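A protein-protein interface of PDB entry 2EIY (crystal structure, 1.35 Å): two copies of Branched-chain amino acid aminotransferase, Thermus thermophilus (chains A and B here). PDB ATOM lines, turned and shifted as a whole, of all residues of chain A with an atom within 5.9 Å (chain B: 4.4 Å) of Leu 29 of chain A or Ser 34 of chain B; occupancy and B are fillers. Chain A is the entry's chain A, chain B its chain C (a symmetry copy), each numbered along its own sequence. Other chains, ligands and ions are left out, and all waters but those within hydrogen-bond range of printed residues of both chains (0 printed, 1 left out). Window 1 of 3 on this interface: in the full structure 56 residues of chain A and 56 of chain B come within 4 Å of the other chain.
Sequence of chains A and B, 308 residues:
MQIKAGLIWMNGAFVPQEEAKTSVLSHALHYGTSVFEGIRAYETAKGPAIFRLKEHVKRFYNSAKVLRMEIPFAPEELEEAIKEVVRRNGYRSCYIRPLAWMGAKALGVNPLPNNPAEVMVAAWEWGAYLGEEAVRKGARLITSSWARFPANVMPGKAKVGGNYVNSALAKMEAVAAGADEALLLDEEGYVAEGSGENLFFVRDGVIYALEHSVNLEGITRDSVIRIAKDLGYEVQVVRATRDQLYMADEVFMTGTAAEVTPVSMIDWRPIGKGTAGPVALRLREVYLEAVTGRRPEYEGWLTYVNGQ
The side-chain hydroxyl (OG) of Ser 34 of chain B sits at hydrogen-bond distance from the backbone carbonyl oxygen (O) of Leu 29 of chain A (2.8 Å). O of Tyr 31 of chain A lies close to O of Gly 161 of chain B.
The backbone carbonyl oxygen (O) of Val 24 of chain A sits at hydrogen-bond distance from a ring nitrogen (NE2) of His 30 of chain A (2.8 Å). OG1 of Thr 33 of chain A sits close to N of Ala 28 of chain A, 3.3 Å away. The backbone NH (N) of Ala 28 of chain A sits at hydrogen-bond distance from the backbone carbonyl oxygen (O) of Met 102 of chain A, 3.1 Å away. The indole nitrogen (NE1) of Trp 101 of chain B lies within hydrogen-bond range of the side-chain hydroxyl (OG1) of Thr 22 of chain B (3.2 Å). The backbone NH (N) of Ala 28 of chain B lies close to the side-chain hydroxyl (OG1) of Thr 33 of chain B (3.3 Å). O of Ser 34 of chain B sits at hydrogen-bond distance from N of Gly 161 of chain B, at 2.7 Å.
Of the 15 printed residues of chain B, 8 touch a printed residue of chain A. Printed residues of chain B that touch a printed residue of chain A: Ala 28, Leu 29, Gly 32, Ser 34, Leu 99, Trp 101, Val 160 and Gly 161. Hydrophobic or aromatic side chains of chain B that line the printed part of chain A: Ala 28, Leu 29, Leu 99, Trp 101 and Val 160. Printed residues of chain A that touch a printed residue of chain B: Val 24, Ala 28, Leu 29, His 30, Tyr 31, Gly 32 and Val 165. Hydrophobic or aromatic side chains of chain A within 4 Å of the printed part of chain B: Val 24, Ala 28, Leu 29, His 30 and Val 165. Along chain A the printed residues that touch a printed residue of chain B span positions 24 to 165.
Leu 29 of chain A touches five residues of chain B. Ser 34 of chain B touches one residue of chain A. Of the printed residues of chain A, Leu 99 of chain B touches Val 24 (3.8 Å), Leu 29 (3.7 Å) and His 30 (3.7 Å). Printed residues of chain A within 4 Å of Leu 29 of chain B: Ala 28 (3.9 Å) and Leu 29 (3.95 Å). Printed residues of chain A within 4 Å of Gly 161 of chain B: His 30, Tyr 31 and Gly 32. Of the printed residues of chain A, Ala 28 of chain B touches Leu 29. Met 69 of chain B touches none of the printed residues of chain A. The nearest residue of chain B that does not touch Leu 29 of chain A is Thr 22 of chain B (4.1 Å). The nearest residue of chain A that does not touch Ser 34 of chain B is His 30 of chain A (4.2 Å).
Ala 28 of chain A touches Leu 29 of chain B, and with the chains exchanged Leu 29 of chain A touches Ala 28 of chain B. Leu 29 of chain A touches its own counterpart, Leu 29 of chain B. Of the 14 pairs that touch across the chains among the printed residues, 3 have their exchanged pair printed and touching as well.
Among the printed residues, merely in contact across the chains: His 30 of chain A with Gly 161 of chain B, Val 165 of chain A with Gly 32 of chain B, Gly 32 of chain A with Gly 161 of chain B, His 30 of chain A with Leu 99 of chain B, Val 24 of chain A with Trp 101 of chain B, Val 165 of chain A with Val 160 of chain B, Leu 29 of chain A with Leu 99 of chain B, Val 24 of chain A with Leu 99 of chain B, Leu 29 of chain A with Ala 28 of chain B, Ala 28 of chain A with Leu 29 of chain B, Leu 29 of chain A with Leu 29 of chain B and Leu 29 of chain A with Trp 101 of chain B.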
ATOM      1  N   SER A  23      18.797   6.589  29.579  1.00  0.00           N
ATOM      2  CA  SER A  23      20.188   6.375  29.971  1.00  0.00           C
ATOM      3  C   SER A  23      20.939   7.671  30.250  1.00  0.00           C
ATOM      4  O   SER A  23      20.760   8.666  29.542  1.00  0.00           O
ATOM      5  CB  SER A  23      20.929   5.602  28.880  1.00  0.00           C
ATOM      6  OG  SER A  23      22.318   5.540  29.163  1.00  0.00           O
ATOM      7  N   VAL A  24      21.781   7.657  31.278  1.00  0.00           N
ATOM      8  CA  VAL A  24      22.570   8.838  31.610  1.00  0.00           C
ATOM      9  C   VAL A  24      23.667   9.015  30.562  1.00  0.00           C
ATOM     10  O   VAL A  24      24.431   9.977  30.612  1.00  0.00           O
ATOM     11  CB  VAL A  24      23.215   8.735  33.017  1.00  0.00           C
ATOM     12  CG1 VAL A  24      22.125   8.712  34.084  1.00  0.00           C
ATOM     13  CG2 VAL A  24      24.084   7.491  33.115  1.00  0.00           C
ATOM     14  N   LEU A  25      23.743   8.081  29.617  1.00  0.00           N
ATOM     15  CA  LEU A  25      24.730   8.162  28.544  1.00  0.00           C
ATOM     16  C   LEU A  25      24.073   8.734  27.287  1.00  0.00           C
ATOM     17  O   LEU A  25      24.645   8.689  26.196  1.00  0.00           O
ATOM     18  CB  LEU A  25      25.324   6.781  28.239  1.00  0.00           C
ATOM     19  CG  LEU A  25      26.107   6.099  29.363  1.00  0.00           C
ATOM     20  CD1 LEU A  25      26.651   4.770  28.861  1.00  0.00           C
ATOM     21  CD2 LEU A  25      27.247   6.997  29.831  1.00  0.00           C
ATOM     22  N   SER A  26      22.866   9.270  27.444  1.00  0.00           N
ATOM     23  CA  SER A  26      22.150   9.866  26.320  1.00  0.00           C
ATOM     24  C   SER A  26      22.883  11.116  25.846  1.00  0.00           C
ATOM     25  O   SER A  26      23.227  11.988  26.645  1.00  0.00           O
ATOM     26  CB  SER A  26      20.719  10.237  26.720  1.00  0.00           C
ATOM     27  OG  SER A  26      19.952   9.080  27.002  1.00  0.00           O
ATOM     28  N   HIS A  27      23.107  11.184  24.539  1.00  0.00           N
ATOM     29  CA  HIS A  27      23.803  12.299  23.897  1.00  0.00           C
ATOM     30  C   HIS A  27      23.262  13.651  24.368  1.00  0.00           C
ATOM     31  O   HIS A  27      24.030  14.559  24.689  1.00  0.00           O
ATOM     32  CB  HIS A  27      23.650  12.162  22.376  1.00  0.00           C
ATOM     33  CG  HIS A  27      24.643  12.951  21.577  1.00  0.00           C
ATOM     34  ND1 HIS A  27      24.451  14.274  21.239  1.00  0.00           N
ATOM     35  CD2 HIS A  27      25.815  12.584  21.005  1.00  0.00           C
ATOM     36  CE1 HIS A  27      25.460  14.686  20.492  1.00  0.00           C
ATOM     37  NE2 HIS A  27      26.301  13.679  20.335  1.00  0.00           N
ATOM     38  N   ALA A  28      21.939  13.778  24.435  1.00  0.00           N
ATOM     39  CA  ALA A  28      21.327  15.039  24.844  1.00  0.00           C
ATOM     40  C   ALA A  28      21.620  15.466  26.279  1.00  0.00           C
ATOM     41  O   ALA A  28      21.587  16.657  26.585  1.00  0.00           O
ATOM     42  CB  ALA A  28      19.820  14.983  24.622  1.00  0.00           C
ATOM     43  N   LEU A  29      21.904  14.512  27.163  1.00  0.00           N
ATOM     44  CA  LEU A  29      22.192  14.856  28.552  1.00  0.00           C
ATOM     45  C   LEU A  29      23.607  15.424  28.680  1.00  0.00           C
ATOM     46  O   LEU A  29      23.921  16.124  29.643  1.00  0.00           O
ATOM     47  CB  LEU A  29      22.040  13.623  29.453  1.00  0.00           C
ATOM     48  CG  LEU A  29      21.887  13.888  30.956  1.00  0.00           C
ATOM     49  CD1 LEU A  29      20.580  14.639  31.209  1.00  0.00           C
ATOM     50  CD2 LEU A  29      21.894  12.567  31.722  1.00  0.00           C
ATOM     51  N   HIS A  30      24.451  15.114  27.700  1.00  0.00           N
ATOM     52  CA  HIS A  30      25.834  15.579  27.685  1.00  0.00           C
ATOM     53  C   HIS A  30      26.089  16.772  26.772  1.00  0.00           C
ATOM     54  O   HIS A  30      26.941  17.612  27.073  1.00  0.00           O
ATOM     55  CB  HIS A  30      26.769  14.458  27.217  1.00  0.00           C
ATOM     56  CG  HIS A  30      26.790  13.263  28.113  1.00  0.00           C
ATOM     57  ND1 HIS A  30      27.915  12.878  28.809  1.00  0.00           N
ATOM     58  CD2 HIS A  30      25.828  12.361  28.420  1.00  0.00           C
ATOM     59  CE1 HIS A  30      27.645  11.789  29.508  1.00  0.00           C
ATOM     60  NE2 HIS A  30      26.386  11.455  29.288  1.00  0.00           N
ATOM     61  N   TYR A  31      25.352  16.844  25.665  1.00  0.00           N
ATOM     62  CA  TYR A  31      25.590  17.883  24.669  1.00  0.00           C
ATOM     63  C   TYR A  31      24.428  18.803  24.274  1.00  0.00           C
ATOM     64  O   TYR A  31      24.528  19.531  23.278  1.00  0.00           O
ATOM     65  CB  TYR A  31      26.170  17.217  23.413  1.00  0.00           C
ATOM     66  CG  TYR A  31      27.333  16.274  23.681  1.00  0.00           C
ATOM     67  CD1 TYR A  31      27.299  14.950  23.232  1.00  0.00           C
ATOM     68  CD2 TYR A  31      28.474  16.705  24.361  1.00  0.00           C
ATOM     69  CE1 TYR A  31      28.372  14.083  23.452  1.00  0.00           C
ATOM     70  CE2 TYR A  31      29.553  15.843  24.586  1.00  0.00           C
ATOM     71  CZ  TYR A  31      29.494  14.535  24.127  1.00  0.00           C
ATOM     72  OH  TYR A  31      30.557  13.682  24.343  1.00  0.00           O
ATOM     73  N   GLY A  32      23.337  18.767  25.037  1.00  0.00           N
ATOM     74  CA  GLY A  32      22.192  19.633  24.773  1.00  0.00           C
ATOM     75  C   GLY A  32      21.420  19.392  23.491  1.00  0.00           C
ATOM     76  O   GLY A  32      20.629  20.235  23.065  1.00  0.00           O
ATOM     77  N   THR A  33      21.623  18.221  22.902  1.00  0.00           N
ATOM     78  CA  THR A  33      20.989  17.853  21.647  1.00  0.00           C
ATOM     79  C   THR A  33      19.564  17.310  21.759  1.00  0.00           C
ATOM     80  O   THR A  33      19.292  16.147  21.454  1.00  0.00           O
ATOM     81  CB  THR A  33      21.875  16.842  20.907  1.00  0.00           C
ATOM     82  OG1 THR A  33      22.326  15.850  21.837  1.00  0.00           O
ATOM     83  CG2 THR A  33      23.093  17.546  20.297  1.00  0.00           C
ATOM     84  N   MET A 102      18.488  13.071  21.526  1.00  0.00           N
ATOM     85  CA  MET A 102      19.423  12.097  20.980  1.00  0.00           C
ATOM     86  C   MET A 102      19.793  11.127  22.093  1.00  0.00           C
ATOM     87  O   MET A 102      20.169  11.539  23.195  1.00  0.00           O
ATOM     88  CB  MET A 102      20.671  12.799  20.435  1.00  0.00           C
ATOM     89  CG  MET A 102      20.385  13.739  19.271  1.00  0.00           C
ATOM     90  SD  MET A 102      19.325  13.004  17.992  1.00  0.00           S
ATOM     91  CE  MET A 102      20.416  11.845  17.261  1.00  0.00           C
ATOM     92  N   VAL A 165      20.798  27.250  28.080  1.00  0.00           N
ATOM     93  CA  VAL A 165      21.836  27.504  29.063  1.00  0.00           C
ATOM     94  C   VAL A 165      21.914  29.036  29.132  1.00  0.00           C
ATOM     95  O   VAL A 165      22.077  29.617  30.206  1.00  0.00           O
ATOM     96  CB  VAL A 165      23.190  26.932  28.605  1.00  0.00           C
ATOM     97  CG1 VAL A 165      24.335  27.604  29.357  1.00  0.00           C
ATOM     98  CG2 VAL A 165      23.212  25.427  28.850  1.00  0.00           C
ATOM     99  N   THR B  22      17.902   8.222  34.157  1.00  0.00           N
ATOM    100  CA  THR B  22      17.372   9.386  34.851  1.00  0.00           C
ATOM    101  C   THR B  22      16.048   9.799  34.209  1.00  0.00           C
ATOM    102  O   THR B  22      15.787   9.481  33.051  1.00  0.00           O
ATOM    103  CB  THR B  22      18.380  10.560  34.788  1.00  0.00           C
ATOM    104  OG1 THR B  22      17.975  11.596  35.690  1.00  0.00           O
ATOM    105  CG2 THR B  22      18.461  11.126  33.376  1.00  0.00           C
ATOM    106  N   ALA B  28      18.308  19.089  32.774  1.00  0.00           N
ATOM    107  CA  ALA B  28      19.400  19.025  31.807  1.00  0.00           C
ATOM    108  C   ALA B  28      19.026  18.426  30.459  1.00  0.00           C
ATOM    109  O   ALA B  28      19.652  18.746  29.450  1.00  0.00           O
ATOM    110  CB  ALA B  28      20.568  18.258  32.401  1.00  0.00           C
ATOM    111  N   LEU B  29      18.022  17.552  30.431  1.00  0.00           N
ATOM    112  CA  LEU B  29      17.617  16.936  29.173  1.00  0.00           C
ATOM    113  C   LEU B  29      16.818  17.927  28.323  1.00  0.00           C
ATOM    114  O   LEU B  29      16.727  17.784  27.105  1.00  0.00           O
ATOM    115  CB  LEU B  29      16.776  15.681  29.439  1.00  0.00           C
ATOM    116  CG  LEU B  29      16.660  14.700  28.266  1.00  0.00           C
ATOM    117  CD1 LEU B  29      18.028  14.090  27.969  1.00  0.00           C
ATOM    118  CD2 LEU B  29      15.657  13.605  28.610  1.00  0.00           C
ATOM    119  N   GLY B  32      19.930  21.763  28.614  1.00  0.00           N
ATOM    120  CA  GLY B  32      21.386  21.699  28.521  1.00  0.00           C
ATOM    121  C   GLY B  32      22.188  22.012  29.773  1.00  0.00           C
ATOM    122  O   GLY B  32      23.401  22.250  29.710  1.00  0.00           O
ATOM    123  N   THR B  33      21.517  21.978  30.917  1.00  0.00           N
ATOM    124  CA  THR B  33      22.133  22.292  32.196  1.00  0.00           C
ATOM    125  C   THR B  33      22.899  21.145  32.863  1.00  0.00           C
ATOM    126  O   THR B  33      22.515  20.640  33.924  1.00  0.00           O
ATOM    127  CB  THR B  33      21.064  22.820  33.147  1.00  0.00           C
ATOM    128  OG1 THR B  33      19.899  21.994  33.034  1.00  0.00           O
ATOM    129  CG2 THR B  33      20.697  24.261  32.784  1.00  0.00           C
ATOM    130  N   SER B  34      23.996  20.746  32.230  1.00  0.00           N
ATOM    131  CA  SER B  34      24.852  19.690  32.750  1.00  0.00           C
ATOM    132  C   SER B  34      26.296  20.120  32.538  1.00  0.00           C
ATOM    133  O   SER B  34      26.564  21.052  31.775  1.00  0.00           O
ATOM    134  CB  SER B  34      24.609  18.380  31.992  1.00  0.00           C
ATOM    135  OG  SER B  34      24.971  18.510  30.624  1.00  0.00           O
ATOM    136  N   VAL B  35      27.215  19.470  33.242  1.00  0.00           N
ATOM    137  CA  VAL B  35      28.639  19.732  33.063  1.00  0.00           C
ATOM    138  C   VAL B  35      29.311  18.371  32.998  1.00  0.00           C
ATOM    139  O   VAL B  35      28.838  17.406  33.602  1.00  0.00           O
ATOM    140  CB  VAL B  35      29.258  20.569  34.214  1.00  0.00           C
ATOM    141  CG1 VAL B  35      28.564  21.915  34.298  1.00  0.00           C
ATOM    142  CG2 VAL B  35      29.174  19.822  35.533  1.00  0.00           C
ATOM    143  N   LEU B  67      27.449  27.503  36.384  1.00  0.00           N
ATOM    144  CA  LEU B  67      25.998  27.334  36.340  1.00  0.00           C
ATOM    145  C   LEU B  67      25.362  27.466  37.719  1.00  0.00           C
ATOM    146  O   LEU B  67      24.148  27.315  37.856  1.00  0.00           O
ATOM    147  CB  LEU B  67      25.633  25.956  35.783  1.00  0.00           C
ATOM    148  CG  LEU B  67      25.958  25.607  34.335  1.00  0.00           C
ATOM    149  CD1 LEU B  67      25.464  24.194  34.048  1.00  0.00           C
ATOM    150  CD2 LEU B  67      25.288  26.601  33.398  1.00  0.00           C
ATOM    151  N   MET B  69      25.680  25.465  39.934  1.00  0.00           N
ATOM    152  CA  MET B  69      25.268  24.090  40.174  1.00  0.00           C
ATOM    153  C   MET B  69      26.009  23.554  41.391  1.00  0.00           C
ATOM    154  O   MET B  69      27.218  23.738  41.521  1.00  0.00           O
ATOM    155  CB  MET B  69      25.609  23.234  38.952  1.00  0.00           C
ATOM    156  CG  MET B  69      25.470  21.735  39.165  1.00  0.00           C
ATOM    157  SD  MET B  69      26.154  20.803  37.780  1.00  0.00           S
ATOM    158  CE  MET B  69      24.818  20.904  36.609  1.00  0.00           C
ATOM    159  N   LEU B  99      29.802  13.182  34.828  1.00  0.00           N
ATOM    160  CA  LEU B  99      28.715  14.064  34.412  1.00  0.00           C
ATOM    161  C   LEU B  99      27.873  14.481  35.605  1.00  0.00           C
ATOM    162  O   LEU B  99      27.504  13.651  36.431  1.00  0.00           O
ATOM    163  CB  LEU B  99      27.805  13.360  33.399  1.00  0.00           C
ATOM    164  CG  LEU B  99      26.549  14.123  32.949  1.00  0.00           C
ATOM    165  CD1 LEU B  99      26.922  15.140  31.872  1.00  0.00           C
ATOM    166  CD2 LEU B  99      25.512  13.146  32.407  1.00  0.00           C
ATOM    167  N   ALA B 100      27.584  15.774  35.695  1.00  0.00           N
ATOM    168  CA  ALA B 100      26.732  16.303  36.754  1.00  0.00           C
ATOM    169  C   ALA B 100      25.604  17.000  36.006  1.00  0.00           C
ATOM    170  O   ALA B 100      25.857  17.785  35.091  1.00  0.00           O
ATOM    171  CB  ALA B 100      27.492  17.295  37.620  1.00  0.00           C
ATOM    172  N   TRP B 101      24.361  16.716  36.375  1.00  0.00           N
ATOM    173  CA  TRP B 101      23.242  17.326  35.674  1.00  0.00           C
ATOM    174  C   TRP B 101      22.100  17.721  36.592  1.00  0.00           C
ATOM    175  O   TRP B 101      21.913  17.135  37.661  1.00  0.00           O
ATOM    176  CB  TRP B 101      22.733  16.370  34.586  1.00  0.00           C
ATOM    177  CG  TRP B 101      21.987  15.156  35.092  1.00  0.00           C
ATOM    178  CD1 TRP B 101      20.632  15.003  35.167  1.00  0.00           C
ATOM    179  CD2 TRP B 101      22.556  13.926  35.564  1.00  0.00           C
ATOM    180  NE1 TRP B 101      20.320  13.751  35.650  1.00  0.00           N
ATOM    181  CE2 TRP B 101      21.483  13.071  35.902  1.00  0.00           C
ATOM    182  CE3 TRP B 101      23.869  13.461  35.732  1.00  0.00           C
ATOM    183  CZ2 TRP B 101      21.680  11.776  36.399  1.00  0.00           C
ATOM    184  CZ3 TRP B 101      24.065  12.171  36.227  1.00  0.00           C
ATOM    185  CH2 TRP B 101      22.973  11.346  36.554  1.00  0.00           C
ATOM    186  N   LYS B 159      32.838  23.153  30.479  1.00  0.00           N
ATOM    187  CA  LYS B 159      32.294  22.080  29.661  1.00  0.00           C
ATOM    188  C   LYS B 159      30.836  21.912  30.078  1.00  0.00           C
ATOM    189  O   LYS B 159      30.477  20.972  30.788  1.00  0.00           O
ATOM    190  CB  LYS B 159      33.074  20.775  29.864  1.00  0.00           C
ATOM    191  CG  LYS B 159      34.373  20.712  29.062  1.00  0.00           C
ATOM    192  CD  LYS B 159      35.223  19.490  29.419  1.00  0.00           C
ATOM    193  CE  LYS B 159      35.683  18.714  28.187  1.00  0.00           C
ATOM    194  NZ  LYS B 159      36.180  19.615  27.134  1.00  0.00           N
ATOM    195  N   VAL B 160      30.014  22.866  29.650  1.00  0.00           N
ATOM    196  CA  VAL B 160      28.584  22.873  29.932  1.00  0.00           C
ATOM    197  C   VAL B 160      27.878  22.193  28.762  1.00  0.00           C
ATOM    198  O   VAL B 160      28.118  22.529  27.601  1.00  0.00           O
ATOM    199  CB  VAL B 160      28.066  24.323  30.096  1.00  0.00           C
ATOM    200  CG1 VAL B 160      26.548  24.347  30.101  1.00  0.00           C
ATOM    201  CG2 VAL B 160      28.600  24.911  31.393  1.00  0.00           C
ATOM    202  N   GLY B 161      27.005  21.240  29.076  1.00  0.00           N
ATOM    203  CA  GLY B 161      26.299  20.501  28.044  1.00  0.00           C
ATOM    204  C   GLY B 161      25.741  21.305  26.883  1.00  0.00           C
ATOM    205  O   GLY B 161      26.018  20.997  25.724  1.00  0.00           O
